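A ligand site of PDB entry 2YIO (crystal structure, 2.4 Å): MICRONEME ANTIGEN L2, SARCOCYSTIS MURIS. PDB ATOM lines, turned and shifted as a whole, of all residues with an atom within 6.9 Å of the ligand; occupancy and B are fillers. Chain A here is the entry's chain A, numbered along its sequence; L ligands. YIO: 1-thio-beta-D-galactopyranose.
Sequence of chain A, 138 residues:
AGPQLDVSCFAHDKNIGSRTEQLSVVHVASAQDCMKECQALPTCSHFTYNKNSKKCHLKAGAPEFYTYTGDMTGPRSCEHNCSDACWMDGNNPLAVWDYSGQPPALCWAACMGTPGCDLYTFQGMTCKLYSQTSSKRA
The side-chain amino group (NZ) of Lys 59 sits at hydrogen-bond distance from an oxygen (O3) of the ligand, 2.9 Å away. The side-chain carboxylate (OD1) of Asp 71 lies within hydrogen-bond range of an oxygen (O6) of the ligand (2.5 Å). O4 of the ligand lies within hydrogen-bond range of OH of Tyr 66 (3.0 Å). O3 of the ligand lies within hydrogen-bond range of O of Ser 18, 3.0 Å away.
The side-chain hydroxyl of Thr 48 sits at hydrogen-bond distance from the side-chain hydroxyl of Thr 73 (3.0 Å). The backbone carbonyl oxygen (O) of Thr 48 lies within hydrogen-bond range of the backbone NH (N) of His 57. The backbone NH (N) of Ile 16 sits at hydrogen-bond distance from the backbone carbonyl oxygen (O) of Asp 71 (3.4 Å). The backbone carbonyl oxygen of Lys 55 is in hydrogen-bond range of the backbone NH of Asn 50 (3.0 Å). The backbone NH (N) of Gly 17 lies within hydrogen-bond range of the backbone carbonyl oxygen (O) of Tyr 66 (2.8 Å). OD1 of Asp 71 lies within hydrogen-bond range of ND2 of Asn 50 (2.8 Å). OG of Ser 18 sits at hydrogen-bond distance from OG1 of Thr 20. OD1 of Asn 50 is in hydrogen-bond range of N of Ser 53 (3.1 Å).
Merely in contact with the ligand: Thr 48 (3.5 Å), Tyr 68 (3.6 Å), His 57 (3.6 Å), Asn 50 (3.7 Å) and Gln 22 (3.96 Å). Hydrophobic or aromatic side chains within 4 Å of the ligand: His 57, Tyr 66 and Tyr 68. Of the 22 residues printed, 9 come within 4 Å of the ligand. The nearest printed residue that does not touch the ligand is Gly 17 (4.3 Å).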
ATOM      1  N   ILE A  16       3.045 -26.533  16.102  1.00  0.00           N
ATOM      2  CA  ILE A  16       2.921 -27.815  15.434  1.00  0.00           C
ATOM      3  C   ILE A  16       1.492 -28.346  15.588  1.00  0.00           C
ATOM      4  O   ILE A  16       1.069 -28.710  16.690  1.00  0.00           O
ATOM      5  CB  ILE A  16       3.944 -28.847  16.007  1.00  0.00           C
ATOM      6  CG1 ILE A  16       5.403 -28.330  15.883  1.00  0.00           C
ATOM      7  CG2 ILE A  16       3.807 -30.183  15.284  1.00  0.00           C
ATOM      8  CD1 ILE A  16       6.344 -28.984  16.914  1.00  0.00           C
ATOM      9  N   GLY A  17       0.750 -28.352  14.493  1.00  0.00           N
ATOM     10  CA  GLY A  17      -0.537 -28.976  14.439  1.00  0.00           C
ATOM     11  C   GLY A  17      -0.529 -30.254  13.647  1.00  0.00           C
ATOM     12  O   GLY A  17       0.484 -30.647  13.117  1.00  0.00           O
ATOM     13  N   SER A  18      -1.674 -30.938  13.610  1.00  0.00           N
ATOM     14  CA  SER A  18      -1.811 -32.166  12.835  1.00  0.00           C
ATOM     15  C   SER A  18      -3.080 -32.052  12.080  1.00  0.00           C
ATOM     16  O   SER A  18      -4.073 -31.667  12.691  1.00  0.00           O
ATOM     17  CB  SER A  18      -1.885 -33.383  13.742  1.00  0.00           C
ATOM     18  OG  SER A  18      -2.209 -34.514  12.978  1.00  0.00           O
ATOM     19  N   ARG A  19      -3.056 -32.367  10.768  1.00  0.00           N
ATOM     20  CA  ARG A  19      -4.270 -32.266   9.941  1.00  0.00           C
ATOM     21  C   ARG A  19      -5.181 -33.464   9.973  1.00  0.00           C
ATOM     22  O   ARG A  19      -6.207 -33.446   9.329  1.00  0.00           O
ATOM     23  CB  ARG A  19      -3.928 -32.027   8.461  1.00  0.00           C
ATOM     24  CG  ARG A  19      -3.082 -30.834   8.190  1.00  0.00           C
ATOM     25  CD  ARG A  19      -3.062 -30.507   6.672  1.00  0.00           C
ATOM     26  NE  ARG A  19      -3.209 -29.058   6.469  1.00  0.00           N
ATOM     27  CZ  ARG A  19      -2.273 -28.251   6.008  1.00  0.00           C
ATOM     28  NH1 ARG A  19      -1.090 -28.693   5.623  1.00  0.00           N
ATOM     29  NH2 ARG A  19      -2.547 -26.965   5.912  1.00  0.00           N
ATOM     30  N   THR A  20      -4.815 -34.520  10.689  1.00  0.00           N
ATOM     31  CA  THR A  20      -5.564 -35.764  10.643  1.00  0.00           C
ATOM     32  C   THR A  20      -7.019 -35.557  11.056  1.00  0.00           C
ATOM     33  O   THR A  20      -7.307 -34.791  11.962  1.00  0.00           O
ATOM     34  CB  THR A  20      -4.945 -36.782  11.592  1.00  0.00           C
ATOM     35  OG1 THR A  20      -3.545 -36.883  11.316  1.00  0.00           O
ATOM     36  CG2 THR A  20      -5.582 -38.152  11.465  1.00  0.00           C
ATOM     37  N   GLU A  21      -7.933 -36.274  10.381  1.00  0.00           N
ATOM     38  CA  GLU A  21      -9.336 -36.227  10.687  1.00  0.00           C
ATOM     39  C   GLU A  21      -9.547 -36.530  12.145  1.00  0.00           C
ATOM     40  O   GLU A  21      -8.923 -37.448  12.703  1.00  0.00           O
ATOM     41  CB  GLU A  21     -10.121 -37.262   9.890  1.00  0.00           C
ATOM     42  CG  GLU A  21      -9.882 -37.191   8.427  1.00  0.00           C
ATOM     43  CD  GLU A  21     -11.075 -36.696   7.630  1.00  0.00           C
ATOM     44  OE1 GLU A  21     -11.924 -37.562   7.287  1.00  0.00           O
ATOM     45  OE2 GLU A  21     -11.102 -35.471   7.309  1.00  0.00           O
ATOM     46  N   GLN A  22     -10.471 -35.816  12.752  1.00  0.00           N
ATOM     47  CA  GLN A  22     -10.738 -36.026  14.153  1.00  0.00           C
ATOM     48  C   GLN A  22     -11.823 -37.004  14.492  1.00  0.00           C
ATOM     49  O   GLN A  22     -12.691 -37.229  13.719  1.00  0.00           O
ATOM     50  CB  GLN A  22     -11.004 -34.719  14.860  1.00  0.00           C
ATOM     51  CG  GLN A  22     -12.090 -33.911  14.346  1.00  0.00           C
ATOM     52  CD  GLN A  22     -11.722 -32.475  14.468  1.00  0.00           C
ATOM     53  OE1 GLN A  22     -10.544 -32.064  14.175  1.00  0.00           O
ATOM     54  NE2 GLN A  22     -12.691 -31.681  14.912  1.00  0.00           N
ATOM     55  N   PHE A  47      -3.280 -35.841  19.587  1.00  0.00           N
ATOM     56  CA  PHE A  47      -4.158 -34.743  19.689  1.00  0.00           C
ATOM     57  C   PHE A  47      -3.461 -33.450  19.356  1.00  0.00           C
ATOM     58  O   PHE A  47      -2.259 -33.296  19.552  1.00  0.00           O
ATOM     59  CB  PHE A  47      -4.709 -34.675  21.112  1.00  0.00           C
ATOM     60  CG  PHE A  47      -3.686 -34.328  22.156  1.00  0.00           C
ATOM     61  CD1 PHE A  47      -3.329 -33.008  22.381  1.00  0.00           C
ATOM     62  CD2 PHE A  47      -3.103 -35.294  22.906  1.00  0.00           C
ATOM     63  CE1 PHE A  47      -2.411 -32.689  23.350  1.00  0.00           C
ATOM     64  CE2 PHE A  47      -2.172 -34.974  23.881  1.00  0.00           C
ATOM     65  CZ  PHE A  47      -1.813 -33.684  24.101  1.00  0.00           C
ATOM     66  N   THR A  48      -4.241 -32.506  18.836  1.00  0.00           N
ATOM     67  CA  THR A  48      -3.778 -31.150  18.689  1.00  0.00           C
ATOM     68  C   THR A  48      -4.595 -30.269  19.613  1.00  0.00           C
ATOM     69  O   THR A  48      -5.846 -30.267  19.561  1.00  0.00           O
ATOM     70  CB  THR A  48      -3.853 -30.678  17.235  1.00  0.00           C
ATOM     71  OG1 THR A  48      -2.981 -31.521  16.448  1.00  0.00           O
ATOM     72  CG2 THR A  48      -3.374 -29.182  17.143  1.00  0.00           C
ATOM     73  N   TYR A  49      -3.859 -29.519  20.440  1.00  0.00           N
ATOM     74  CA  TYR A  49      -4.430 -28.492  21.336  1.00  0.00           C
ATOM     75  C   TYR A  49      -3.908 -27.115  20.977  1.00  0.00           C
ATOM     76  O   TYR A  49      -2.716 -26.920  20.749  1.00  0.00           O
ATOM     77  CB  TYR A  49      -4.037 -28.789  22.762  1.00  0.00           C
ATOM     78  CG  TYR A  49      -4.512 -27.778  23.792  1.00  0.00           C
ATOM     79  CD1 TYR A  49      -5.872 -27.611  24.056  1.00  0.00           C
ATOM     80  CD2 TYR A  49      -3.605 -27.018  24.526  1.00  0.00           C
ATOM     81  CE1 TYR A  49      -6.305 -26.713  25.001  1.00  0.00           C
ATOM     82  CE2 TYR A  49      -4.043 -26.113  25.466  1.00  0.00           C
ATOM     83  CZ  TYR A  49      -5.397 -25.971  25.703  1.00  0.00           C
ATOM     84  OH  TYR A  49      -5.826 -25.114  26.668  1.00  0.00           O
ATOM     85  N   ASN A  50      -4.817 -26.148  20.888  1.00  0.00           N
ATOM     86  CA  ASN A  50      -4.435 -24.761  20.566  1.00  0.00           C
ATOM     87  C   ASN A  50      -4.505 -23.875  21.776  1.00  0.00           C
ATOM     88  O   ASN A  50      -5.542 -23.754  22.347  1.00  0.00           O
ATOM     89  CB  ASN A  50      -5.311 -24.229  19.453  1.00  0.00           C
ATOM     90  CG  ASN A  50      -4.782 -22.896  18.886  1.00  0.00           C
ATOM     91  OD1 ASN A  50      -4.933 -21.831  19.497  1.00  0.00           O
ATOM     92  ND2 ASN A  50      -4.160 -22.957  17.717  1.00  0.00           N
ATOM     93  N   SER A  53      -7.204 -20.532  21.204  1.00  0.00           N
ATOM     94  CA  SER A  53      -8.557 -20.956  20.957  1.00  0.00           C
ATOM     95  C   SER A  53      -9.048 -21.952  22.041  1.00  0.00           C
ATOM     96  O   SER A  53     -10.236 -22.104  22.265  1.00  0.00           O
ATOM     97  CB  SER A  53      -8.495 -21.649  19.610  1.00  0.00           C
ATOM     98  OG  SER A  53      -9.650 -22.356  19.354  1.00  0.00           O
ATOM     99  N   LYS A  55      -9.210 -25.095  21.759  1.00  0.00           N
ATOM    100  CA  LYS A  55      -9.840 -26.259  21.157  1.00  0.00           C
ATOM    101  C   LYS A  55      -8.843 -27.372  21.282  1.00  0.00           C
ATOM    102  O   LYS A  55      -7.631 -27.165  21.120  1.00  0.00           O
ATOM    103  CB  LYS A  55     -10.190 -26.043  19.676  1.00  0.00           C
ATOM    104  CG  LYS A  55     -11.231 -25.020  19.405  1.00  0.00           C
ATOM    105  CD  LYS A  55     -11.716 -25.137  17.960  1.00  0.00           C
ATOM    106  CE  LYS A  55     -12.172 -23.802  17.370  1.00  0.00           C
ATOM    107  NZ  LYS A  55     -12.870 -23.959  16.047  1.00  0.00           N
ATOM    108  N   HIS A  57      -8.458 -31.329  19.805  1.00  0.00           N
ATOM    109  CA  HIS A  57      -8.865 -32.183  18.690  1.00  0.00           C
ATOM    110  C   HIS A  57      -8.230 -33.540  18.830  1.00  0.00           C
ATOM    111  O   HIS A  57      -7.003 -33.687  18.709  1.00  0.00           O
ATOM    112  CB  HIS A  57      -8.400 -31.592  17.346  1.00  0.00           C
ATOM    113  CG  HIS A  57      -8.908 -30.204  17.063  1.00  0.00           C
ATOM    114  ND1 HIS A  57      -8.234 -29.066  17.464  1.00  0.00           N
ATOM    115  CD2 HIS A  57      -9.984 -29.780  16.374  1.00  0.00           C
ATOM    116  CE1 HIS A  57      -8.897 -27.995  17.032  1.00  0.00           C
ATOM    117  NE2 HIS A  57      -9.954 -28.406  16.359  1.00  0.00           N
ATOM    118  N   LYS A  59      -7.606 -37.381  17.647  1.00  0.00           N
ATOM    119  CA  LYS A  59      -7.442 -37.984  16.295  1.00  0.00           C
ATOM    120  C   LYS A  59      -7.030 -39.448  16.378  1.00  0.00           C
ATOM    121  O   LYS A  59      -6.325 -39.861  17.325  1.00  0.00           O
ATOM    122  CB  LYS A  59      -6.405 -37.205  15.526  1.00  0.00           C
ATOM    123  CG  LYS A  59      -6.760 -35.743  15.336  1.00  0.00           C
ATOM    124  CD  LYS A  59      -5.573 -34.869  15.308  1.00  0.00           C
ATOM    125  CE  LYS A  59      -5.954 -33.375  15.065  1.00  0.00           C
ATOM    126  NZ  LYS A  59      -6.384 -32.964  13.671  1.00  0.00           N
ATOM    127  N   TYR A  66       1.822 -30.065  10.502  1.00  0.00           N
ATOM    128  CA  TYR A  66       1.790 -28.800   9.749  1.00  0.00           C
ATOM    129  C   TYR A  66       1.828 -27.627  10.731  1.00  0.00           C
ATOM    130  O   TYR A  66       1.807 -27.832  11.931  1.00  0.00           O
ATOM    131  CB  TYR A  66       0.572 -28.751   8.836  1.00  0.00           C
ATOM    132  CG  TYR A  66      -0.690 -28.218   9.462  1.00  0.00           C
ATOM    133  CD1 TYR A  66      -1.328 -28.921  10.479  1.00  0.00           C
ATOM    134  CD2 TYR A  66      -1.266 -27.026   9.025  1.00  0.00           C
ATOM    135  CE1 TYR A  66      -2.483 -28.438  11.067  1.00  0.00           C
ATOM    136  CE2 TYR A  66      -2.456 -26.534   9.604  1.00  0.00           C
ATOM    137  CZ  TYR A  66      -3.035 -27.242  10.630  1.00  0.00           C
ATOM    138  OH  TYR A  66      -4.177 -26.796  11.208  1.00  0.00           O
ATOM    139  N   TYR A  68       0.489 -24.178  12.440  1.00  0.00           N
ATOM    140  CA  TYR A  68      -0.692 -23.395  12.738  1.00  0.00           C
ATOM    141  C   TYR A  68      -0.473 -22.750  14.083  1.00  0.00           C
ATOM    142  O   TYR A  68      -0.114 -23.428  15.057  1.00  0.00           O
ATOM    143  CB  TYR A  68      -1.932 -24.260  12.805  1.00  0.00           C
ATOM    144  CG  TYR A  68      -3.204 -23.445  12.992  1.00  0.00           C
ATOM    145  CD1 TYR A  68      -3.579 -22.981  14.264  1.00  0.00           C
ATOM    146  CD2 TYR A  68      -4.011 -23.124  11.902  1.00  0.00           C
ATOM    147  CE1 TYR A  68      -4.746 -22.232  14.461  1.00  0.00           C
ATOM    148  CE2 TYR A  68      -5.195 -22.353  12.086  1.00  0.00           C
ATOM    149  CZ  TYR A  68      -5.550 -21.926  13.364  1.00  0.00           C
ATOM    150  OH  TYR A  68      -6.675 -21.179  13.572  1.00  0.00           O
ATOM    151  N   THR A  69      -0.698 -21.438  14.135  1.00  0.00           N
ATOM    152  CA  THR A  69      -0.242 -20.604  15.245  1.00  0.00           C
ATOM    153  C   THR A  69      -0.984 -20.983  16.533  1.00  0.00           C
ATOM    154  O   THR A  69      -2.197 -21.048  16.557  1.00  0.00           O
ATOM    155  CB  THR A  69      -0.446 -19.081  14.886  1.00  0.00           C
ATOM    156  OG1 THR A  69       0.396 -18.765  13.764  1.00  0.00           O
ATOM    157  CG2 THR A  69      -0.117 -18.131  16.105  1.00  0.00           C
ATOM    158  N   GLY A  70      -0.225 -21.269  17.580  1.00  0.00           N
ATOM    159  CA  GLY A  70      -0.782 -21.709  18.851  1.00  0.00           C
ATOM    160  C   GLY A  70      -0.991 -23.211  19.054  1.00  0.00           C
ATOM    161  O   GLY A  70      -1.184 -23.663  20.201  1.00  0.00           O
ATOM    162  N   ASP A  71      -0.901 -24.012  17.991  1.00  0.00           N
ATOM    163  CA  ASP A  71      -1.020 -25.472  18.121  1.00  0.00           C
ATOM    164  C   ASP A  71       0.129 -26.129  18.840  1.00  0.00           C
ATOM    165  O   ASP A  71       1.254 -25.678  18.811  1.00  0.00           O
ATOM    166  CB  ASP A  71      -1.146 -26.144  16.750  1.00  0.00           C
ATOM    167  CG  ASP A  71      -2.549 -26.109  16.210  1.00  0.00           C
ATOM    168  OD1 ASP A  71      -3.444 -25.519  16.875  1.00  0.00           O
ATOM    169  OD2 ASP A  71      -2.744 -26.680  15.107  1.00  0.00           O
ATOM    170  N   MET A  72      -0.188 -27.246  19.475  1.00  0.00           N
ATOM    171  CA  MET A  72       0.804 -28.210  19.917  1.00  0.00           C
ATOM    172  C   MET A  72       0.193 -29.588  19.667  1.00  0.00           C
ATOM    173  O   MET A  72      -1.048 -29.743  19.691  1.00  0.00           O
ATOM    174  CB  MET A  72       1.172 -27.995  21.374  1.00  0.00           C
ATOM    175  CG  MET A  72      -0.006 -28.142  22.324  1.00  0.00           C
ATOM    176  SD  MET A  72       0.393 -27.496  23.960  1.00  0.00           S
ATOM    177  CE  MET A  72      -0.158 -25.806  23.732  1.00  0.00           C
ATOM    178  N   THR A  73       1.054 -30.585  19.426  1.00  0.00           N
ATOM    179  CA  THR A  73       0.605 -31.913  19.118  1.00  0.00           C
ATOM    180  C   THR A  73       1.284 -32.920  20.029  1.00  0.00           C
ATOM    181  O   THR A  73       2.493 -32.929  20.174  1.00  0.00           O
ATOM    182  CB  THR A  73       0.773 -32.179  17.646  1.00  0.00           C
ATOM    183  OG1 THR A  73      -0.024 -31.195  16.951  1.00  0.00           O
ATOM    184  CG2 THR A  73       0.317 -33.606  17.271  1.00  0.00           C
HETATM  185  C1  YIO L   1      -8.113 -27.874  12.440  1.00  0.00           C
HETATM  186  C2  YIO L   1      -7.110 -29.066  12.637  1.00  0.00           C
HETATM  187  C3  YIO L   1      -6.737 -29.139  14.143  1.00  0.00           C
HETATM  188  C4  YIO L   1      -5.972 -27.916  14.545  1.00  0.00           C
HETATM  189  C5  YIO L   1      -6.867 -26.716  14.118  1.00  0.00           C
HETATM  190  C6  YIO L   1      -6.293 -25.429  14.624  1.00  0.00           C
HETATM  191  O2  YIO L   1      -7.620 -30.322  12.149  1.00  0.00           O
HETATM  192  O3  YIO L   1      -5.965 -30.246  14.535  1.00  0.00           O
HETATM  193  O4  YIO L   1      -4.669 -27.908  13.936  1.00  0.00           O
HETATM  194  O5  YIO L   1      -7.164 -26.778  12.686  1.00  0.00           O
HETATM  195  O6  YIO L   1      -5.676 -25.742  15.886  1.00  0.00           O
HETATM  196  S1  YIO L   1      -9.211 -27.490  10.955  1.00  0.00           S
